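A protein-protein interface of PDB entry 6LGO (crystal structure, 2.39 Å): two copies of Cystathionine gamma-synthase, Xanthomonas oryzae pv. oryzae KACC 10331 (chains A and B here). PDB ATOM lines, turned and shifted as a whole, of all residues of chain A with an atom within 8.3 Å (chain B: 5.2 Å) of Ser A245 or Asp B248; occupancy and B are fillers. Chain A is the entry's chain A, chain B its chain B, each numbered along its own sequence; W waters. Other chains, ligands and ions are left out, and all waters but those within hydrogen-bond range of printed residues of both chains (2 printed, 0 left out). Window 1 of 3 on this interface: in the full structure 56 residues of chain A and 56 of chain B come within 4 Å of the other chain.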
ATOM      1  N   ILE A  38     -28.859  11.690  34.654  1.00  0.00           N
ATOM      2  CA  ILE A  38     -28.712  12.580  33.478  1.00  0.00           C
ATOM      3  C   ILE A  38     -27.429  13.403  33.664  1.00  0.00           C
ATOM      4  O   ILE A  38     -27.382  14.245  34.568  1.00  0.00           O
ATOM      5  CB  ILE A  38     -29.947  13.467  33.310  1.00  0.00           C
ATOM      6  CG1 ILE A  38     -31.251  12.662  33.358  1.00  0.00           C
ATOM      7  CG2 ILE A  38     -29.787  14.317  32.035  1.00  0.00           C
ATOM      8  CD1 ILE A  38     -32.506  13.583  33.347  1.00  0.00           C
ATOM      9  N   VAL A  39     -26.438  13.176  32.811  1.00  0.00           N
ATOM     10  CA  VAL A  39     -25.179  13.965  32.883  1.00  0.00           C
ATOM     11  C   VAL A  39     -25.265  15.115  31.889  1.00  0.00           C
ATOM     12  O   VAL A  39     -24.890  14.902  30.714  1.00  0.00           O
ATOM     13  CB  VAL A  39     -23.990  13.031  32.543  1.00  0.00           C
ATOM     14  CG1 VAL A  39     -22.655  13.742  32.631  1.00  0.00           C
ATOM     15  CG2 VAL A  39     -24.014  11.857  33.498  1.00  0.00           C
ATOM     16  N   LEU A  40     -25.777  16.234  32.321  1.00  0.00           N
ATOM     17  CA  LEU A  40     -25.934  17.474  31.489  1.00  0.00           C
ATOM     18  C   LEU A  40     -24.607  18.215  31.333  1.00  0.00           C
ATOM     19  O   LEU A  40     -24.468  18.973  30.369  1.00  0.00           O
ATOM     20  CB  LEU A  40     -26.959  18.400  32.144  1.00  0.00           C
ATOM     21  CG  LEU A  40     -28.381  17.921  32.311  1.00  0.00           C
ATOM     22  CD1 LEU A  40     -29.193  19.019  32.944  1.00  0.00           C
ATOM     23  CD2 LEU A  40     -29.015  17.594  30.994  1.00  0.00           C
ATOM     24  N   THR A  58     -18.782  17.538  26.259  1.00  0.00           N
ATOM     25  CA  THR A  58     -20.079  16.900  25.900  1.00  0.00           C
ATOM     26  C   THR A  58     -20.288  16.958  24.372  1.00  0.00           C
ATOM     27  O   THR A  58     -20.917  16.003  23.885  1.00  0.00           O
ATOM     28  CB  THR A  58     -21.234  17.421  26.769  1.00  0.00           C
ATOM     29  OG1 THR A  58     -21.188  16.695  27.993  1.00  0.00           O
ATOM     30  CG2 THR A  58     -22.581  17.248  26.113  1.00  0.00           C
ATOM     31  N   ASN A  62     -20.455  12.180  25.621  1.00  0.00           N
ATOM     32  CA  ASN A  62     -21.147  12.298  26.930  1.00  0.00           C
ATOM     33  C   ASN A  62     -21.758  10.938  27.265  1.00  0.00           C
ATOM     34  O   ASN A  62     -22.221  10.196  26.362  1.00  0.00           O
ATOM     35  CB  ASN A  62     -22.190  13.392  26.795  1.00  0.00           C
ATOM     36  CG  ASN A  62     -23.163  13.444  27.933  1.00  0.00           C
ATOM     37  OD1 ASN A  62     -24.052  12.579  27.967  1.00  0.00           O
ATOM     38  ND2 ASN A  62     -23.054  14.494  28.774  1.00  0.00           N
ATOM     39  N   THR A  64     -24.384   9.943  29.017  1.00  0.00           N
ATOM     40  CA  THR A  64     -25.832   9.698  28.862  1.00  0.00           C
ATOM     41  C   THR A  64     -26.145   9.449  27.378  1.00  0.00           C
ATOM     42  O   THR A  64     -26.881   8.482  27.027  1.00  0.00           O
ATOM     43  CB  THR A  64     -26.638  10.856  29.446  1.00  0.00           C
ATOM     44  OG1 THR A  64     -26.311  10.986  30.826  1.00  0.00           O
ATOM     45  CG2 THR A  64     -28.115  10.599  29.250  1.00  0.00           C
ATOM     46  N   ARG A  65     -25.578  10.253  26.501  1.00  0.00           N
ATOM     47  CA  ARG A  65     -25.771  10.069  25.054  1.00  0.00           C
ATOM     48  C   ARG A  65     -25.150   8.735  24.630  1.00  0.00           C
ATOM     49  O   ARG A  65     -25.694   8.055  23.740  1.00  0.00           O
ATOM     50  CB  ARG A  65     -25.097  11.240  24.353  1.00  0.00           C
ATOM     51  CG  ARG A  65     -25.542  11.366  22.908  1.00  0.00           C
ATOM     52  CD  ARG A  65     -25.207  12.705  22.302  1.00  0.00           C
ATOM     53  NE  ARG A  65     -23.793  12.772  22.132  1.00  0.00           N
ATOM     54  CZ  ARG A  65     -23.075  13.834  22.529  1.00  0.00           C
ATOM     55  NH1 ARG A  65     -23.667  14.917  22.981  1.00  0.00           N
ATOM     56  NH2 ARG A  65     -21.771  13.831  22.378  1.00  0.00           N
ATOM     57  N   LEU A  68     -27.427   5.640  24.926  1.00  0.00           N
ATOM     58  CA  LEU A  68     -28.333   5.521  23.767  1.00  0.00           C
ATOM     59  C   LEU A  68     -27.556   5.044  22.549  1.00  0.00           C
ATOM     60  O   LEU A  68     -28.040   4.086  21.912  1.00  0.00           O
ATOM     61  CB  LEU A  68     -29.009   6.850  23.507  1.00  0.00           C
ATOM     62  CG  LEU A  68     -29.961   6.868  22.296  1.00  0.00           C
ATOM     63  CD1 LEU A  68     -31.077   5.858  22.550  1.00  0.00           C
ATOM     64  CD2 LEU A  68     -30.548   8.272  22.118  1.00  0.00           C
ATOM     65  N   ILE A  83     -25.289   9.916  18.211  1.00  0.00           N
ATOM     66  CA  ILE A  83     -26.583  10.551  18.480  1.00  0.00           C
ATOM     67  C   ILE A  83     -26.480  12.027  18.097  1.00  0.00           C
ATOM     68  O   ILE A  83     -25.616  12.742  18.639  1.00  0.00           O
ATOM     69  CB  ILE A  83     -27.021  10.340  19.928  1.00  0.00           C
ATOM     70  CG1 ILE A  83     -26.918   8.875  20.363  1.00  0.00           C
ATOM     71  CG2 ILE A  83     -28.432  10.893  20.133  1.00  0.00           C
ATOM     72  CD1 ILE A  83     -27.700   7.927  19.528  1.00  0.00           C
ATOM     73  N   THR A  84     -27.302  12.452  17.145  1.00  0.00           N
ATOM     74  CA  THR A  84     -27.278  13.820  16.545  1.00  0.00           C
ATOM     75  C   THR A  84     -28.492  14.604  17.086  1.00  0.00           C
ATOM     76  O   THR A  84     -29.383  13.953  17.557  1.00  0.00           O
ATOM     77  CB  THR A  84     -27.337  13.702  15.029  1.00  0.00           C
ATOM     78  OG1 THR A  84     -28.501  12.950  14.665  1.00  0.00           O
ATOM     79  CG2 THR A  84     -26.081  13.029  14.528  1.00  0.00           C
ATOM     80  N   SER A  85     -28.518  15.924  16.954  1.00  0.00           N
ATOM     81  CA  SER A  85     -29.613  16.839  17.376  1.00  0.00           C
ATOM     82  C   SER A  85     -30.921  16.499  16.644  1.00  0.00           C
ATOM     83  O   SER A  85     -32.001  16.750  17.232  1.00  0.00           O
ATOM     84  CB  SER A  85     -29.259  18.263  17.116  1.00  0.00           C
ATOM     85  OG  SER A  85     -28.775  18.348  15.764  1.00  0.00           O
ATOM     86  N   THR A  86     -30.860  16.020  15.408  1.00  0.00           N
ATOM     87  CA  THR A  86     -32.051  15.679  14.577  1.00  0.00           C
ATOM     88  C   THR A  86     -31.712  14.489  13.669  1.00  0.00           C
ATOM     89  O   THR A  86     -30.524  14.154  13.495  1.00  0.00           O
ATOM     90  CB  THR A  86     -32.542  16.883  13.737  1.00  0.00           C
ATOM     91  OG1 THR A  86     -31.585  17.097  12.685  1.00  0.00           O
ATOM     92  CG2 THR A  86     -32.695  18.147  14.568  1.00  0.00           C
ATOM     93  N   VAL A 217     -39.126  14.652  21.675  1.00  0.00           N
ATOM     94  CA  VAL A 217     -37.684  14.731  21.357  1.00  0.00           C
ATOM     95  C   VAL A 217     -37.567  14.773  19.836  1.00  0.00           C
ATOM     96  O   VAL A 217     -38.272  13.979  19.215  1.00  0.00           O
ATOM     97  CB  VAL A 217     -36.909  13.511  21.886  1.00  0.00           C
ATOM     98  CG1 VAL A 217     -35.469  13.602  21.384  1.00  0.00           C
ATOM     99  CG2 VAL A 217     -36.914  13.386  23.393  1.00  0.00           C
ATOM    100  N   VAL A 218     -36.717  15.632  19.284  1.00  0.00           N
ATOM    101  CA  VAL A 218     -36.252  15.515  17.885  1.00  0.00           C
ATOM    102  C   VAL A 218     -34.795  15.113  18.044  1.00  0.00           C
ATOM    103  O   VAL A 218     -34.154  15.642  18.926  1.00  0.00           O
ATOM    104  CB  VAL A 218     -36.432  16.838  17.130  1.00  0.00           C
ATOM    105  CG1 VAL A 218     -35.955  16.761  15.738  1.00  0.00           C
ATOM    106  CG2 VAL A 218     -37.870  17.246  17.109  1.00  0.00           C
ATOM    107  N   GLY A 219     -34.396  14.053  17.372  1.00  0.00           N
ATOM    108  CA  GLY A 219     -33.069  13.462  17.413  1.00  0.00           C
ATOM    109  C   GLY A 219     -32.798  12.545  16.241  1.00  0.00           C
ATOM    110  O   GLY A 219     -33.752  12.080  15.539  1.00  0.00           O
ATOM    111  N   LEU A 242     -22.670  18.400  15.597  1.00  0.00           N
ATOM    112  CA  LEU A 242     -24.008  17.814  15.230  1.00  0.00           C
ATOM    113  C   LEU A 242     -24.523  16.992  16.395  1.00  0.00           C
ATOM    114  O   LEU A 242     -25.571  16.423  16.246  1.00  0.00           O
ATOM    115  CB  LEU A 242     -23.840  16.821  14.034  1.00  0.00           C
ATOM    116  CG  LEU A 242     -23.584  17.506  12.708  1.00  0.00           C
ATOM    117  CD1 LEU A 242     -23.265  16.538  11.600  1.00  0.00           C
ATOM    118  CD2 LEU A 242     -24.837  18.264  12.324  1.00  0.00           C
ATOM    119  N   THR A 243     -23.736  16.770  17.430  1.00  0.00           N
ATOM    120  CA  THR A 243     -24.145  15.944  18.564  1.00  0.00           C
ATOM    121  C   THR A 243     -25.344  16.542  19.305  1.00  0.00           C
ATOM    122  O   THR A 243     -25.485  17.737  19.424  1.00  0.00           O
ATOM    123  CB  THR A 243     -22.992  15.683  19.538  1.00  0.00           C
ATOM    124  OG1 THR A 243     -22.270  16.883  19.823  1.00  0.00           O
ATOM    125  CG2 THR A 243     -22.100  14.601  18.977  1.00  0.00           C
ATOM    126  N   GLY A 244     -26.129  15.603  19.829  1.00  0.00           N
ATOM    127  CA  GLY A 244     -27.380  15.773  20.592  1.00  0.00           C
ATOM    128  C   GLY A 244     -27.166  16.205  22.040  1.00  0.00           C
ATOM    129  O   GLY A 244     -26.184  15.841  22.657  1.00  0.00           O
ATOM    130  N   SER A 245     -28.198  16.791  22.584  1.00  0.00           N
ATOM    131  CA  SER A 245     -28.352  17.130  24.023  1.00  0.00           C
ATOM    132  C   SER A 245     -28.513  15.877  24.914  1.00  0.00           C
ATOM    133  O   SER A 245     -29.190  14.912  24.570  1.00  0.00           O
ATOM    134  CB  SER A 245     -29.467  18.083  24.180  1.00  0.00           C
ATOM    135  OG  SER A 245     -30.360  17.637  25.168  1.00  0.00           O
ATOM    136  N   PRO A 246     -27.813  15.825  26.057  1.00  0.00           N
ATOM    137  CA  PRO A 246     -27.947  14.698  26.968  1.00  0.00           C
ATOM    138  C   PRO A 246     -29.384  14.528  27.500  1.00  0.00           C
ATOM    139  O   PRO A 246     -29.773  13.400  27.732  1.00  0.00           O
ATOM    140  CB  PRO A 246     -26.934  15.031  28.059  1.00  0.00           C
ATOM    141  CG  PRO A 246     -25.870  15.833  27.321  1.00  0.00           C
ATOM    142  CD  PRO A 246     -26.678  16.695  26.394  1.00  0.00           C
ATOM    143  N   PHE A 247     -30.130  15.620  27.694  1.00  0.00           N
ATOM    144  CA  PHE A 247     -31.487  15.513  28.219  1.00  0.00           C
ATOM    145  C   PHE A 247     -32.298  14.721  27.191  1.00  0.00           C
ATOM    146  O   PHE A 247     -32.987  13.800  27.603  1.00  0.00           O
ATOM    147  CB  PHE A 247     -32.095  16.869  28.522  1.00  0.00           C
ATOM    148  CG  PHE A 247     -33.507  16.761  29.057  1.00  0.00           C
ATOM    149  CD1 PHE A 247     -33.721  16.433  30.356  1.00  0.00           C
ATOM    150  CD2 PHE A 247     -34.583  16.922  28.229  1.00  0.00           C
ATOM    151  CE1 PHE A 247     -34.996  16.297  30.850  1.00  0.00           C
ATOM    152  CE2 PHE A 247     -35.856  16.734  28.700  1.00  0.00           C
ATOM    153  CZ  PHE A 247     -36.060  16.466  30.024  1.00  0.00           C
ATOM    154  N   ASP A 248     -32.195  15.073  25.916  1.00  0.00           N
ATOM    155  CA  ASP A 248     -32.881  14.358  24.818  1.00  0.00           C
ATOM    156  C   ASP A 248     -32.460  12.872  24.782  1.00  0.00           C
ATOM    157  O   ASP A 248     -33.370  12.019  24.619  1.00  0.00           O
ATOM    158  CB  ASP A 248     -32.703  15.039  23.453  1.00  0.00           C
ATOM    159  CG  ASP A 248     -33.458  16.352  23.335  1.00  0.00           C
ATOM    160  OD1 ASP A 248     -33.992  16.771  24.396  1.00  0.00           O
ATOM    161  OD2 ASP A 248     -33.598  16.913  22.129  1.00  0.00           O
ATOM    162  N   ALA A 249     -31.191  12.556  25.015  1.00  0.00           N
ATOM    163  CA  ALA A 249     -30.702  11.159  25.051  1.00  0.00           C
ATOM    164  C   ALA A 249     -31.386  10.424  26.194  1.00  0.00           C
ATOM    165  O   ALA A 249     -31.761   9.284  26.035  1.00  0.00           O
ATOM    166  CB  ALA A 249     -29.203  11.073  25.193  1.00  0.00           C
ATOM    167  N   PHE A 250     -31.487  11.062  27.326  1.00  0.00           N
ATOM    168  CA  PHE A 250     -32.191  10.533  28.495  1.00  0.00           C
ATOM    169  C   PHE A 250     -33.646  10.189  28.103  1.00  0.00           C
ATOM    170  O   PHE A 250     -34.109   9.055  28.391  1.00  0.00           O
ATOM    171  CB  PHE A 250     -32.101  11.512  29.653  1.00  0.00           C
ATOM    172  CG  PHE A 250     -33.207  11.288  30.647  1.00  0.00           C
ATOM    173  CD1 PHE A 250     -33.114  10.261  31.543  1.00  0.00           C
ATOM    174  CD2 PHE A 250     -34.302  12.099  30.689  1.00  0.00           C
ATOM    175  CE1 PHE A 250     -34.160   9.981  32.401  1.00  0.00           C
ATOM    176  CE2 PHE A 250     -35.358  11.816  31.544  1.00  0.00           C
ATOM    177  CZ  PHE A 250     -35.290  10.750  32.378  1.00  0.00           C
ATOM    178  N   LEU A 251     -34.392  11.108  27.528  1.00  0.00           N
ATOM    179  CA  LEU A 251     -35.802  10.809  27.235  1.00  0.00           C
ATOM    180  C   LEU A 251     -35.909   9.736  26.156  1.00  0.00           C
ATOM    181  O   LEU A 251     -36.872   8.940  26.182  1.00  0.00           O
ATOM    182  CB  LEU A 251     -36.506  12.053  26.733  1.00  0.00           C
ATOM    183  CG  LEU A 251     -36.940  13.042  27.822  1.00  0.00           C
ATOM    184  CD1 LEU A 251     -37.588  14.300  27.193  1.00  0.00           C
ATOM    185  CD2 LEU A 251     -37.949  12.384  28.788  1.00  0.00           C
ATOM    186  N   THR A 252     -35.007   9.812  25.169  1.00  0.00           N
ATOM    187  CA  THR A 252     -34.955   8.854  24.083  1.00  0.00           C
ATOM    188  C   THR A 252     -34.698   7.461  24.691  1.00  0.00           C
ATOM    189  O   THR A 252     -35.429   6.576  24.363  1.00  0.00           O
ATOM    190  CB  THR A 252     -33.962   9.294  23.008  1.00  0.00           C
ATOM    191  OG1 THR A 252     -34.337  10.538  22.442  1.00  0.00           O
ATOM    192  CG2 THR A 252     -33.983   8.317  21.849  1.00  0.00           C
ATOM    193  N   SER B  85     -27.400  23.018  18.064  1.00  0.00           N
ATOM    194  CA  SER B  85     -27.095  22.012  19.118  1.00  0.00           C
ATOM    195  C   SER B  85     -25.748  22.327  19.816  1.00  0.00           C
ATOM    196  O   SER B  85     -25.581  21.941  20.994  1.00  0.00           O
ATOM    197  CB  SER B  85     -27.039  20.637  18.577  1.00  0.00           C
ATOM    198  OG  SER B  85     -26.197  20.647  17.426  1.00  0.00           O
ATOM    199  N   VAL B 217     -25.166  22.886  29.605  1.00  0.00           N
ATOM    200  CA  VAL B 217     -25.712  22.974  28.235  1.00  0.00           C
ATOM    201  C   VAL B 217     -24.545  23.168  27.253  1.00  0.00           C
ATOM    202  O   VAL B 217     -23.666  23.988  27.558  1.00  0.00           O
ATOM    203  CB  VAL B 217     -26.688  24.148  28.107  1.00  0.00           C
ATOM    204  CG1 VAL B 217     -27.089  24.292  26.655  1.00  0.00           C
ATOM    205  CG2 VAL B 217     -27.916  24.001  28.973  1.00  0.00           C
ATOM    206  N   VAL B 218     -24.515  22.412  26.153  1.00  0.00           N
ATOM    207  CA  VAL B 218     -23.661  22.736  24.989  1.00  0.00           C
ATOM    208  C   VAL B 218     -24.657  23.254  23.961  1.00  0.00           C
ATOM    209  O   VAL B 218     -25.692  22.641  23.810  1.00  0.00           O
ATOM    210  CB  VAL B 218     -22.888  21.492  24.502  1.00  0.00           C
ATOM    211  CG1 VAL B 218     -22.073  21.798  23.275  1.00  0.00           C
ATOM    212  CG2 VAL B 218     -21.968  20.964  25.575  1.00  0.00           C
ATOM    213  N   SER B 245     -32.121  21.449  21.004  1.00  0.00           N
ATOM    214  CA  SER B 245     -33.206  20.919  21.857  1.00  0.00           C
ATOM    215  C   SER B 245     -33.894  22.033  22.682  1.00  0.00           C
ATOM    216  O   SER B 245     -33.279  22.981  23.167  1.00  0.00           O
ATOM    217  CB  SER B 245     -32.683  19.798  22.685  1.00  0.00           C
ATOM    218  OG  SER B 245     -32.748  20.134  24.041  1.00  0.00           O
ATOM    219  N   PRO B 246     -35.231  21.980  22.757  1.00  0.00           N
ATOM    220  CA  PRO B 246     -35.998  22.917  23.556  1.00  0.00           C
ATOM    221  C   PRO B 246     -35.606  22.884  25.043  1.00  0.00           C
ATOM    222  O   PRO B 246     -35.549  23.893  25.651  1.00  0.00           O
ATOM    223  CB  PRO B 246     -37.430  22.462  23.326  1.00  0.00           C
ATOM    224  CG  PRO B 246     -37.372  21.947  21.907  1.00  0.00           C
ATOM    225  CD  PRO B 246     -36.075  21.159  21.883  1.00  0.00           C
ATOM    226  N   PHE B 247     -35.242  21.745  25.585  1.00  0.00           N
ATOM    227  CA  PHE B 247     -34.871  21.699  26.998  1.00  0.00           C
ATOM    228  C   PHE B 247     -33.656  22.594  27.184  1.00  0.00           C
ATOM    229  O   PHE B 247     -33.627  23.352  28.133  1.00  0.00           O
ATOM    230  CB  PHE B 247     -34.628  20.269  27.452  1.00  0.00           C
ATOM    231  CG  PHE B 247     -34.234  20.195  28.912  1.00  0.00           C
ATOM    232  CD1 PHE B 247     -35.185  20.304  29.876  1.00  0.00           C
ATOM    233  CD2 PHE B 247     -32.928  20.075  29.281  1.00  0.00           C
ATOM    234  CE1 PHE B 247     -34.836  20.289  31.206  1.00  0.00           C
ATOM    235  CE2 PHE B 247     -32.580  20.101  30.607  1.00  0.00           C
ATOM    236  CZ  PHE B 247     -33.540  20.170  31.575  1.00  0.00           C
ATOM    237  N   ASP B 248     -32.664  22.425  26.320  1.00  0.00           N
ATOM    238  CA  ASP B 248     -31.395  23.169  26.370  1.00  0.00           C
ATOM    239  C   ASP B 248     -31.676  24.664  26.175  1.00  0.00           C
ATOM    240  O   ASP B 248     -31.051  25.440  26.863  1.00  0.00           O
ATOM    241  CB  ASP B 248     -30.368  22.641  25.371  1.00  0.00           C
ATOM    242  CG  ASP B 248     -29.710  21.335  25.747  1.00  0.00           C
ATOM    243  OD1 ASP B 248     -30.239  20.711  26.719  1.00  0.00           O
ATOM    244  OD2 ASP B 248     -28.617  20.940  25.068  1.00  0.00           O
ATOM    245  N   ALA B 249     -32.638  25.054  25.347  1.00  0.00           N
ATOM    246  CA  ALA B 249     -33.007  26.473  25.180  1.00  0.00           C
ATOM    247  C   ALA B 249     -33.615  26.977  26.483  1.00  0.00           C
ATOM    248  O   ALA B 249     -33.364  28.089  26.847  1.00  0.00           O
ATOM    249  CB  ALA B 249     -33.966  26.660  24.066  1.00  0.00           C
ATOM    250  N   PHE B 250     -34.377  26.152  27.153  1.00  0.00           N
ATOM    251  CA  PHE B 250     -35.007  26.525  28.411  1.00  0.00           C
ATOM    252  C   PHE B 250     -33.874  26.819  29.413  1.00  0.00           C
ATOM    253  O   PHE B 250     -33.904  27.881  30.067  1.00  0.00           O
ATOM    254  CB  PHE B 250     -36.001  25.460  28.858  1.00  0.00           C
ATOM    255  CG  PHE B 250     -36.168  25.487  30.355  1.00  0.00           C
ATOM    256  CD1 PHE B 250     -37.008  26.406  30.932  1.00  0.00           C
ATOM    257  CD2 PHE B 250     -35.518  24.583  31.159  1.00  0.00           C
ATOM    258  CE1 PHE B 250     -37.121  26.458  32.308  1.00  0.00           C
ATOM    259  CE2 PHE B 250     -35.555  24.705  32.529  1.00  0.00           C
ATOM    260  CZ  PHE B 250     -36.354  25.639  33.097  1.00  0.00           C
ATOM    261  N   LEU B 251     -32.904  25.940  29.567  1.00  0.00           N
ATOM    262  CA  LEU B 251     -31.867  26.172  30.584  1.00  0.00           C
ATOM    263  C   LEU B 251     -31.004  27.360  30.184  1.00  0.00           C
ATOM    264  O   LEU B 251     -30.498  28.084  31.098  1.00  0.00           O
ATOM    265  CB  LEU B 251     -30.955  24.957  30.701  1.00  0.00           C
ATOM    266  CG  LEU B 251     -31.476  23.793  31.546  1.00  0.00           C
ATOM    267  CD1 LEU B 251     -30.474  22.605  31.533  1.00  0.00           C
ATOM    268  CD2 LEU B 251     -31.744  24.241  32.983  1.00  0.00           C
ATOM    269  N   THR B 252     -30.748  27.486  28.878  1.00  0.00           N
ATOM    270  CA  THR B 252     -29.944  28.590  28.361  1.00  0.00           C
ATOM    271  C   THR B 252     -30.695  29.900  28.675  1.00  0.00           C
ATOM    272  O   THR B 252     -30.057  30.792  29.221  1.00  0.00           O
ATOM    273  CB  THR B 252     -29.556  28.372  26.897  1.00  0.00           C
ATOM    274  OG1 THR B 252     -28.836  27.158  26.686  1.00  0.00           O
ATOM    275  CG2 THR B 252     -28.655  29.495  26.416  1.00  0.00           C
ATOM    276  N   LEU B 253     -31.987  30.007  28.331  1.00  0.00           N
ATOM    277  CA  LEU B 253     -32.767  31.231  28.652  1.00  0.00           C
ATOM    278  C   LEU B 253     -32.700  31.500  30.185  1.00  0.00           C
ATOM    279  O   LEU B 253     -32.424  32.614  30.658  1.00  0.00           O
ATOM    280  CB  LEU B 253     -34.181  31.054  28.125  1.00  0.00           C
ATOM    281  CG  LEU B 253     -35.014  32.332  28.070  1.00  0.00           C
ATOM    282  CD1 LEU B 253     -34.556  33.220  26.966  1.00  0.00           C
ATOM    283  CD2 LEU B 253     -36.463  32.046  27.845  1.00  0.00           C
HETATM  284  O   HOH W   1     -35.497  19.171  24.287  1.00  0.00           O
HETATM  285  O   HOH W   2     -28.998  18.318  27.559  1.00  0.00           O
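The side-chain hydroxyl of Ser A245 lies within hydrogen-bond range of the side-chain carboxylate of Asp B248, at 3.4 Å.
Ser B85 touches its own counterpart, Ser A85. Ser A245 touches its own counterpart, Ser B245. Ser A245 touches Asp B248, and with the chains exchanged Asp A248 touches Ser B245. Phe A247 touches its own counterpart, Phe B247.
Of the 12 printed residues of chain B, 5 touch a printed residue of chain A. Hydrophobic or aromatic side chains of chain B within 4 Å of the printed part of chain A: Val B218 and Phe B247. Among the printed residues, 7 pairs touch across the chains.
Water W2 lies within hydrogen-bond range of OD1 of Asp B248, OG of Ser A245 and N of Phe A247. Water W1 lies within hydrogen-bond range of the side-chain carboxylate of Asp A248 (2.8 Å), the backbone NH of Phe B247 (2.9 Å) and the side-chain hydroxyl of Ser B245 (2.9 Å).
The backbone carbonyl oxygen of Thr A58 sits at hydrogen-bond distance from the guanidinium group of Arg A65 (2.8 Å). O of Asp A248 sits at hydrogen-bond distance from OG1 of Thr A252 (2.8 Å). The side-chain hydroxyl of Thr A58 sits at hydrogen-bond distance from the side-chain amide nitrogen of Asn A62, 3.0 Å away. The backbone NH (N) of Ser A85 lies within hydrogen-bond range of the backbone carbonyl oxygen (O) of Leu A242, 3.1 Å away. OG of Ser B245 sits at hydrogen-bond distance from N of Asp B248 (3.2 Å). N of Asp A248 sits at hydrogen-bond distance from OG of Ser A245.
Among the printed residues, merely in contact across the chains: Thr A58 with Val B218, Ser A85 with Ser B85, Thr A243 with Ser B85, Ser A245 with Ser B245, Phe A247 with Phe B247 and Asp A248 with Ser B245.
Printed residues of chain B within 4 Å of Thr A58: Val B218 (3.8 Å). Printed residues of chain B within 4 Å of Ser A85: Ser B85. Printed residues of chain B within 4 Å of Thr A243: Ser B85 (3.4 Å). Of chain B, only Ser B245 and Asp B248 come within 4 Å of Ser A245. Printed residues of chain A within 4 Å of Ser B85: Ser A85 and Thr A243. Printed residues of chain A within 4 Å of Phe B247: Phe A247 (3.4 Å). Printed residues of chain A within 4 Å of Asp B248: Ser A245. The nearest printed residue of chain B that does not touch Ser A245 is Phe B247 (5.4 Å). The nearest residue of chain A that does not touch Asp B248 is Phe A247 (4.6 Å). The nearest printed residue of chain A that does not touch Ser B245 is Phe A247 (5.6 Å).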
